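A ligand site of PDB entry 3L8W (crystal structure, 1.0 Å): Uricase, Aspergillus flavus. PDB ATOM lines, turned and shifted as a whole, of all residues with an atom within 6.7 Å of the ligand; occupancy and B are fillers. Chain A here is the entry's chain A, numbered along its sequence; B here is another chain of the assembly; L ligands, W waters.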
ATOM      1  N   SER A 158     -21.230   3.298  -7.869  1.00  0.00           N
ATOM      2  CA  SER A 158     -20.718   4.455  -7.161  1.00  0.00           C
ATOM      3  C   SER A 158     -19.197   4.308  -7.153  1.00  0.00           C
ATOM      4  O   SER A 158     -18.674   3.244  -6.890  1.00  0.00           O
ATOM      5  CB  SER A 158     -21.259   4.554  -5.740  1.00  0.00           C
ATOM      6  OG  SER A 158     -20.627   5.597  -4.987  1.00  0.00           O
ATOM      7  N   GLN A 159     -18.499   5.418  -7.437  1.00  0.00           N
ATOM      8  CA  GLN A 159     -17.074   5.472  -7.498  1.00  0.00           C
ATOM      9  C   GLN A 159     -16.561   6.703  -6.713  1.00  0.00           C
ATOM     10  O   GLN A 159     -17.288   7.674  -6.505  1.00  0.00           O
ATOM     11  CB  GLN A 159     -16.609   5.595  -8.960  1.00  0.00           C
ATOM     12  CG  GLN A 159     -17.249   4.531  -9.867  1.00  0.00           C
ATOM     13  CD  GLN A 159     -16.748   4.614 -11.283  1.00  0.00           C
ATOM     14  OE1 GLN A 159     -15.590   4.908 -11.555  1.00  0.00           O
ATOM     15  NE2 GLN A 159     -17.649   4.358 -12.208  1.00  0.00           N
ATOM     16  N   PHE A 160     -15.287   6.700  -6.322  1.00  0.00           N
ATOM     17  CA  PHE A 160     -14.661   7.900  -5.752  1.00  0.00           C
ATOM     18  C   PHE A 160     -13.149   7.775  -5.881  1.00  0.00           C
ATOM     19  O   PHE A 160     -12.455   7.095  -5.121  1.00  0.00           O
ATOM     20  CB  PHE A 160     -15.056   8.157  -4.280  1.00  0.00           C
ATOM     21  CG  PHE A 160     -14.640   9.527  -3.815  1.00  0.00           C
ATOM     22  CD1 PHE A 160     -15.181  10.637  -4.484  1.00  0.00           C
ATOM     23  CD2 PHE A 160     -13.780   9.707  -2.765  1.00  0.00           C
ATOM     24  CE1 PHE A 160     -14.821  11.889  -4.048  1.00  0.00           C
ATOM     25  CE2 PHE A 160     -13.379  10.968  -2.319  1.00  0.00           C
ATOM     26  CZ  PHE A 160     -13.933  12.077  -2.993  1.00  0.00           C
ATOM     27  N   PHE A 163      -9.353  12.311  -6.142  1.00  0.00           N
ATOM     28  CA  PHE A 163      -9.356  13.365  -5.122  1.00  0.00           C
ATOM     29  C   PHE A 163      -7.931  13.768  -4.750  1.00  0.00           C
ATOM     30  O   PHE A 163      -6.965  13.055  -5.009  1.00  0.00           O
ATOM     31  CB  PHE A 163     -10.196  12.972  -3.905  1.00  0.00           C
ATOM     32  CG  PHE A 163      -9.813  11.592  -3.354  1.00  0.00           C
ATOM     33  CD1 PHE A 163     -10.488  10.467  -3.797  1.00  0.00           C
ATOM     34  CD2 PHE A 163      -8.822  11.466  -2.426  1.00  0.00           C
ATOM     35  CE1 PHE A 163     -10.158   9.212  -3.270  1.00  0.00           C
ATOM     36  CE2 PHE A 163      -8.499  10.232  -1.881  1.00  0.00           C
ATOM     37  CZ  PHE A 163      -9.179   9.128  -2.330  1.00  0.00           C
ATOM     38  N   LEU A 171      -7.019   7.600   2.475  1.00  0.00           N
ATOM     39  CA  LEU A 171      -8.116   6.934   1.787  1.00  0.00           C
ATOM     40  C   LEU A 171      -7.705   6.379   0.429  1.00  0.00           C
ATOM     41  O   LEU A 171      -7.138   7.064  -0.417  1.00  0.00           O
ATOM     42  CB  LEU A 171      -9.246   7.948   1.527  1.00  0.00           C
ATOM     43  CG  LEU A 171     -10.528   7.424   0.865  1.00  0.00           C
ATOM     44  CD1 LEU A 171     -11.218   6.419   1.775  1.00  0.00           C
ATOM     45  CD2 LEU A 171     -11.473   8.551   0.497  1.00  0.00           C
ATOM     46  N   ARG A 177     -18.025   1.110  -5.024  1.00  0.00           N
ATOM     47  CA  ARG A 177     -18.317   1.174  -3.598  1.00  0.00           C
ATOM     48  C   ARG A 177     -19.810   1.216  -3.421  1.00  0.00           C
ATOM     49  O   ARG A 177     -20.576   1.474  -4.365  1.00  0.00           O
ATOM     50  CB  ARG A 177     -17.667   2.396  -2.954  1.00  0.00           C
ATOM     51  CG  ARG A 177     -18.200   3.743  -3.448  1.00  0.00           C
ATOM     52  CD  ARG A 177     -17.623   4.938  -2.730  1.00  0.00           C
ATOM     53  NE  ARG A 177     -18.317   6.136  -3.199  1.00  0.00           N
ATOM     54  CZ  ARG A 177     -18.162   7.365  -2.707  1.00  0.00           C
ATOM     55  NH1 ARG A 177     -17.246   7.471  -1.800  1.00  0.00           N
ATOM     56  NH2 ARG A 177     -18.899   8.371  -3.122  1.00  0.00           N
ATOM     57  N   LEU A 179     -22.977   3.244  -1.925  1.00  0.00           N
ATOM     58  CA  LEU A 179     -23.346   4.611  -1.589  1.00  0.00           C
ATOM     59  C   LEU A 179     -24.702   4.583  -0.901  1.00  0.00           C
ATOM     60  O   LEU A 179     -25.695   4.073  -1.468  1.00  0.00           O
ATOM     61  CB  LEU A 179     -23.436   5.483  -2.853  1.00  0.00           C
ATOM     62  CG  LEU A 179     -23.896   6.910  -2.613  1.00  0.00           C
ATOM     63  CD1 LEU A 179     -22.997   7.675  -1.609  1.00  0.00           C
ATOM     64  CD2 LEU A 179     -23.978   7.658  -3.938  1.00  0.00           C
ATOM     65  N   SER A 225     -22.137   6.978 -10.336  1.00  0.00           N
ATOM     66  CA  SER A 225     -21.787   8.195  -9.641  1.00  0.00           C
ATOM     67  C   SER A 225     -20.289   8.430  -9.478  1.00  0.00           C
ATOM     68  O   SER A 225     -19.566   7.577  -8.951  1.00  0.00           O
ATOM     69  CB  SER A 225     -22.432   8.108  -8.244  1.00  0.00           C
ATOM     70  OG  SER A 225     -21.955   9.145  -7.384  1.00  0.00           O
ATOM     71  N   ALA A 226     -19.787   9.595  -9.863  1.00  0.00           N
ATOM     72  CA  ALA A 226     -18.408   9.984  -9.689  1.00  0.00           C
ATOM     73  C   ALA A 226     -18.098  10.506  -8.276  1.00  0.00           C
ATOM     74  O   ALA A 226     -16.923  10.532  -7.845  1.00  0.00           O
ATOM     75  CB  ALA A 226     -18.057  11.059 -10.703  1.00  0.00           C
ATOM     76  N   SER A 227     -19.123  10.915  -7.546  1.00  0.00           N
ATOM     77  CA  SER A 227     -19.059  11.483  -6.203  1.00  0.00           C
ATOM     78  C   SER A 227     -20.469  11.846  -5.794  1.00  0.00           C
ATOM     79  O   SER A 227     -21.377  11.998  -6.643  1.00  0.00           O
ATOM     80  CB  SER A 227     -18.183  12.738  -6.028  1.00  0.00           C
ATOM     81  OG  SER A 227     -18.689  13.838  -6.747  1.00  0.00           O
ATOM     82  N   VAL A 228     -20.675  12.036  -4.513  1.00  0.00           N
ATOM     83  CA  VAL A 228     -21.954  12.559  -4.011  1.00  0.00           C
ATOM     84  C   VAL A 228     -22.205  13.959  -4.627  1.00  0.00           C
ATOM     85  O   VAL A 228     -23.306  14.230  -5.076  1.00  0.00           O
ATOM     86  CB  VAL A 228     -21.978  12.603  -2.477  1.00  0.00           C
ATOM     87  CG1 VAL A 228     -23.266  13.235  -1.990  1.00  0.00           C
ATOM     88  CG2 VAL A 228     -21.843  11.198  -1.894  1.00  0.00           C
ATOM     89  N   GLN A 229     -21.162  14.762  -4.666  1.00  0.00           N
ATOM     90  CA  GLN A 229     -21.212  16.093  -5.250  1.00  0.00           C
ATOM     91  C   GLN A 229     -21.813  16.076  -6.660  1.00  0.00           C
ATOM     92  O   GLN A 229     -22.730  16.836  -6.999  1.00  0.00           O
ATOM     93  CB  GLN A 229     -19.797  16.696  -5.268  1.00  0.00           C
ATOM     94  CG  GLN A 229     -19.168  17.115  -3.955  1.00  0.00           C
ATOM     95  CD  GLN A 229     -18.480  16.042  -3.138  1.00  0.00           C
ATOM     96  OE1 GLN A 229     -18.694  14.832  -3.283  1.00  0.00           O
ATOM     97  NE2 GLN A 229     -17.609  16.461  -2.218  1.00  0.00           N
ATOM     98  N   ASN A 255     -22.756  10.979   3.717  1.00  0.00           N
ATOM     99  CA  ASN A 255     -22.195   9.792   3.096  1.00  0.00           C
ATOM    100  C   ASN A 255     -22.053   8.782   4.245  1.00  0.00           C
ATOM    101  O   ASN A 255     -21.191   8.949   5.095  1.00  0.00           O
ATOM    102  CB  ASN A 255     -20.883  10.090   2.404  1.00  0.00           C
ATOM    103  CG  ASN A 255     -20.418   8.982   1.500  1.00  0.00           C
ATOM    104  OD1 ASN A 255     -21.062   7.956   1.349  1.00  0.00           O
ATOM    105  ND2 ASN A 255     -19.294   9.199   0.845  1.00  0.00           N
ATOM    106  N   HIS A 257     -21.051   5.685   5.579  1.00  0.00           N
ATOM    107  CA  HIS A 257     -20.008   4.790   5.042  1.00  0.00           C
ATOM    108  C   HIS A 257     -20.252   3.327   5.391  1.00  0.00           C
ATOM    109  O   HIS A 257     -20.660   3.013   6.529  1.00  0.00           O
ATOM    110  CB  HIS A 257     -18.644   5.204   5.610  1.00  0.00           C
ATOM    111  CG  HIS A 257     -18.290   6.648   5.332  1.00  0.00           C
ATOM    112  ND1 HIS A 257     -18.132   7.165   4.072  1.00  0.00           N
ATOM    113  CD2 HIS A 257     -18.126   7.682   6.177  1.00  0.00           C
ATOM    114  CE1 HIS A 257     -17.863   8.468   4.174  1.00  0.00           C
ATOM    115  NE2 HIS A 257     -17.844   8.831   5.456  1.00  0.00           N
ATOM    116  N   GLY A 287     -19.301  11.537   6.111  1.00  0.00           N
ATOM    117  CA  GLY A 287     -19.170  12.704   5.234  1.00  0.00           C
ATOM    118  C   GLY A 287     -20.490  13.454   5.231  1.00  0.00           C
ATOM    119  O   GLY A 287     -21.574  12.891   5.432  1.00  0.00           O
ATOM    120  N   ILE A 289     -22.205  16.453   2.664  1.00  0.00           N
ATOM    121  CA  ILE A 289     -22.014  17.167   1.378  1.00  0.00           C
ATOM    122  C   ILE A 289     -23.239  18.011   1.130  1.00  0.00           C
ATOM    123  O   ILE A 289     -24.365  17.530   1.162  1.00  0.00           O
ATOM    124  CB  ILE A 289     -21.814  16.172   0.217  1.00  0.00           C
ATOM    125  CG1 ILE A 289     -20.813  15.042   0.557  1.00  0.00           C
ATOM    126  CG2 ILE A 289     -21.431  16.868  -1.054  1.00  0.00           C
ATOM    127  CD1 ILE A 289     -19.493  15.362   1.103  1.00  0.00           C
ATOM    128  N   TYR B   9     -18.644  21.111   2.221  1.00  0.00           N
ATOM    129  CA  TYR B   9     -18.616  19.651   2.415  1.00  0.00           C
ATOM    130  C   TYR B   9     -17.533  19.385   3.460  1.00  0.00           C
ATOM    131  O   TYR B   9     -16.555  20.125   3.651  1.00  0.00           O
ATOM    132  CB  TYR B   9     -18.413  18.916   1.049  1.00  0.00           C
ATOM    133  CG  TYR B   9     -16.931  18.898   0.784  1.00  0.00           C
ATOM    134  CD1 TYR B   9     -16.231  20.066   0.414  1.00  0.00           C
ATOM    135  CD2 TYR B   9     -16.167  17.753   1.049  1.00  0.00           C
ATOM    136  CE1 TYR B   9     -14.877  20.056   0.225  1.00  0.00           C
ATOM    137  CE2 TYR B   9     -14.832  17.747   0.928  1.00  0.00           C
ATOM    138  CZ  TYR B   9     -14.197  18.894   0.493  1.00  0.00           C
ATOM    139  OH  TYR B   9     -12.816  18.911   0.411  1.00  0.00           O
ATOM    140  N   GLY B  10     -17.630  18.211   4.094  1.00  0.00           N
ATOM    141  CA  GLY B  10     -16.607  17.801   5.038  1.00  0.00           C
ATOM    142  C   GLY B  10     -17.042  16.588   5.841  1.00  0.00           C
ATOM    143  O   GLY B  10     -17.761  15.734   5.332  1.00  0.00           O
ATOM    144  N   LYS B  11     -16.499  16.553   7.086  1.00  0.00           N
ATOM    145  CA  LYS B  11     -16.746  15.381   7.929  1.00  0.00           C
ATOM    146  C   LYS B  11     -17.485  15.850   9.193  1.00  0.00           C
ATOM    147  O   LYS B  11     -17.053  16.782   9.856  1.00  0.00           O
ATOM    148  CB  LYS B  11     -15.483  14.643   8.354  1.00  0.00           C
ATOM    149  CG  LYS B  11     -15.772  13.222   8.878  1.00  0.00           C
ATOM    150  CD  LYS B  11     -16.178  12.227   7.794  1.00  0.00           C
ATOM    151  CE  LYS B  11     -15.095  11.305   7.331  1.00  0.00           C
ATOM    152  NZ  LYS B  11     -15.444  10.625   6.040  1.00  0.00           N
ATOM    153  N   ASN B  52     -12.826  15.648  -9.166  1.00  0.00           N
ATOM    154  CA  ASN B  52     -12.530  15.420  -7.772  1.00  0.00           C
ATOM    155  C   ASN B  52     -11.182  15.983  -7.341  1.00  0.00           C
ATOM    156  O   ASN B  52     -10.832  15.962  -6.144  1.00  0.00           O
ATOM    157  CB  ASN B  52     -12.638  13.920  -7.443  1.00  0.00           C
ATOM    158  CG  ASN B  52     -14.063  13.418  -7.497  1.00  0.00           C
ATOM    159  OD1 ASN B  52     -14.992  14.194  -7.235  1.00  0.00           O
ATOM    160  ND2 ASN B  52     -14.239  12.141  -7.778  1.00  0.00           N
ATOM    161  N   ILE B  55     -11.207  18.237  -4.364  1.00  0.00           N
ATOM    162  CA  ILE B  55     -11.752  17.716  -3.105  1.00  0.00           C
ATOM    163  C   ILE B  55     -10.626  17.214  -2.188  1.00  0.00           C
ATOM    164  O   ILE B  55      -9.925  16.262  -2.547  1.00  0.00           O
ATOM    165  CB  ILE B  55     -12.794  16.611  -3.363  1.00  0.00           C
ATOM    166  CG1 ILE B  55     -14.023  17.075  -4.149  1.00  0.00           C
ATOM    167  CG2 ILE B  55     -13.204  15.980  -2.021  1.00  0.00           C
ATOM    168  CD1 ILE B  55     -14.951  15.908  -4.526  1.00  0.00           C
ATOM    169  N   VAL B  56     -10.503  17.854  -1.038  1.00  0.00           N
ATOM    170  CA  VAL B  56      -9.757  17.330   0.134  1.00  0.00           C
ATOM    171  C   VAL B  56     -10.715  16.270   0.679  1.00  0.00           C
ATOM    172  O   VAL B  56     -11.831  16.608   1.173  1.00  0.00           O
ATOM    173  CB  VAL B  56      -9.432  18.411   1.152  1.00  0.00           C
ATOM    174  CG1 VAL B  56      -8.809  17.841   2.408  1.00  0.00           C
ATOM    175  CG2 VAL B  56      -8.516  19.510   0.577  1.00  0.00           C
ATOM    176  N   ALA B  57     -10.383  14.992   0.613  1.00  0.00           N
ATOM    177  CA  ALA B  57     -11.349  13.957   0.983  1.00  0.00           C
ATOM    178  C   ALA B  57     -11.828  14.144   2.420  1.00  0.00           C
ATOM    179  O   ALA B  57     -11.061  14.549   3.318  1.00  0.00           O
ATOM    180  CB  ALA B  57     -10.693  12.600   0.864  1.00  0.00           C
ATOM    181  N   THR B  58     -13.103  13.815   2.625  1.00  0.00           N
ATOM    182  CA  THR B  58     -13.618  13.974   3.995  1.00  0.00           C
ATOM    183  C   THR B  58     -12.843  13.075   4.960  1.00  0.00           C
ATOM    184  O   THR B  58     -12.659  13.439   6.132  1.00  0.00           O
ATOM    185  CB  THR B  58     -15.133  13.730   4.073  1.00  0.00           C
ATOM    186  OG1 THR B  58     -15.434  12.345   3.843  1.00  0.00           O
ATOM    187  CG2 THR B  58     -15.873  14.577   3.041  1.00  0.00           C
ATOM    188  N   ASP B  59     -12.369  11.902   4.487  1.00  0.00           N
ATOM    189  CA  ASP B  59     -11.531  11.061   5.346  1.00  0.00           C
ATOM    190  C   ASP B  59     -10.268  11.766   5.798  1.00  0.00           C
ATOM    191  O   ASP B  59      -9.762  11.589   6.906  1.00  0.00           O
ATOM    192  CB  ASP B  59     -11.228   9.775   4.589  1.00  0.00           C
ATOM    193  CG  ASP B  59     -10.515   8.791   5.476  1.00  0.00           C
ATOM    194  OD1 ASP B  59     -11.228   8.140   6.288  1.00  0.00           O
ATOM    195  OD2 ASP B  59      -9.302   8.640   5.359  1.00  0.00           O
ATOM    196  N   SER B  60      -9.691  12.555   4.868  1.00  0.00           N
ATOM    197  CA  SER B  60      -8.477  13.341   5.193  1.00  0.00           C
ATOM    198  C   SER B  60      -8.755  14.454   6.200  1.00  0.00           C
ATOM    199  O   SER B  60      -7.925  14.801   7.053  1.00  0.00           O
ATOM    200  CB  SER B  60      -7.892  13.956   3.909  1.00  0.00           C
ATOM    201  OG  SER B  60      -7.634  12.881   2.992  1.00  0.00           O
HETATM  202  N1  LIG L   1     -15.282  10.230   0.477  1.00  0.00           N
HETATM  203  C1  LIG L   1     -16.022  10.914  -0.380  1.00  0.00           C
HETATM  204  N2  LIG L   1     -17.071  10.676  -1.174  1.00  0.00           N
HETATM  205  C2  LIG L   1     -17.700  11.478  -2.007  1.00  0.00           C
HETATM  206  O1  LIG L   1     -18.563  11.138  -2.772  1.00  0.00           O
HETATM  207  N3  LIG L   1     -17.339  12.798  -1.793  1.00  0.00           N
HETATM  208  C3  LIG L   1     -16.307  13.269  -0.953  1.00  0.00           C
HETATM  209  O2  LIG L   1     -16.093  14.469  -0.829  1.00  0.00           O
HETATM  210  C4  LIG L   1     -15.647  12.257  -0.183  1.00  0.00           C
HETATM  211  N4  LIG L   1     -14.542  12.393   0.588  1.00  0.00           N
HETATM  212  C5  LIG L   1     -14.332  11.098   1.015  1.00  0.00           C
HETATM  213  O   HOH W   1     -15.519   7.488   1.208  1.00  0.00           O
HETATM  214  O   HOH W   2     -17.790  11.771   2.214  1.00  0.00           O
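Water W1 lies within hydrogen-bond range of N1 of the ligand (2.8 Å) and NH1 of Arg 177 (3.5 Å).
Water W2 lies within hydrogen-bond range of OG1 of Thr 58 of chain B (2.9 Å), ND2 of Asn 255 (3.3 Å) and N1 of the ligand (3.4 Å).
NH2 of Arg 177 sits at hydrogen-bond distance from O1 of the ligand, 2.8 Å away.
The side-chain amide oxygen (OE1) of Gln 229 sits at hydrogen-bond distance from a nitrogen (N3) of the ligand (2.9 Å).
The backbone NH (N) of Thr 58 of chain B lies within hydrogen-bond range of a nitrogen (N4) of the ligand (2.9 Å).
OG1 of Thr 58 of chain B lies close to N4 of the ligand (3.4 Å).
N of Val 228 is in hydrogen-bond range of O1 of the ligand (2.9 Å).
The side-chain amide nitrogen (ND2) of Asn 255 lies close to a nitrogen (N2) of the ligand (3.3 Å).
The backbone carbonyl oxygen (O) of Ser 158 lies within hydrogen-bond range of the backbone NH (N) of Arg 177.
The backbone NH (N) of Gln 229 lies close to the side-chain hydroxyl (OG) of Ser 227 (3.4 Å).
The side-chain hydroxyl (OG1) of Thr 58 of chain B sits at hydrogen-bond distance from the side-chain amino group (NZ) of Lys 11 of chain B.
The backbone carbonyl oxygen of Asn 255 lies within hydrogen-bond range of a ring nitrogen (NE2) of His 257, 3.4 Å away.
The backbone NH of Asn 255 lies within hydrogen-bond range of the backbone carbonyl oxygen of Gly 287, at 2.8 Å.
O of Ser 227 lies within hydrogen-bond range of OG of Ser 225 (3.0 Å).
O of Val 56 of chain B sits at hydrogen-bond distance from OH of Tyr 9 of chain B (2.6 Å).
Residues that only touch the ligand: Phe 160, Ile 55 of chain B, Ser 227, Ala 57 of chain B, Tyr 9 of chain B and Leu 171.
Hydrophobic or aromatic side chains that line the ligand: Phe 160, Leu 171, Val 228, Tyr 9 of chain B, Ile 55 of chain B and Ala 57 of chain B.
11 residues have an atom within 4 Å of the ligand: Phe 160, Leu 171, Arg 177, Ser 227, Val 228, Gln 229, Asn 255, Tyr 9 of chain B, Ile 55 of chain B, Ala 57 of chain B and Thr 58 of chain B.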
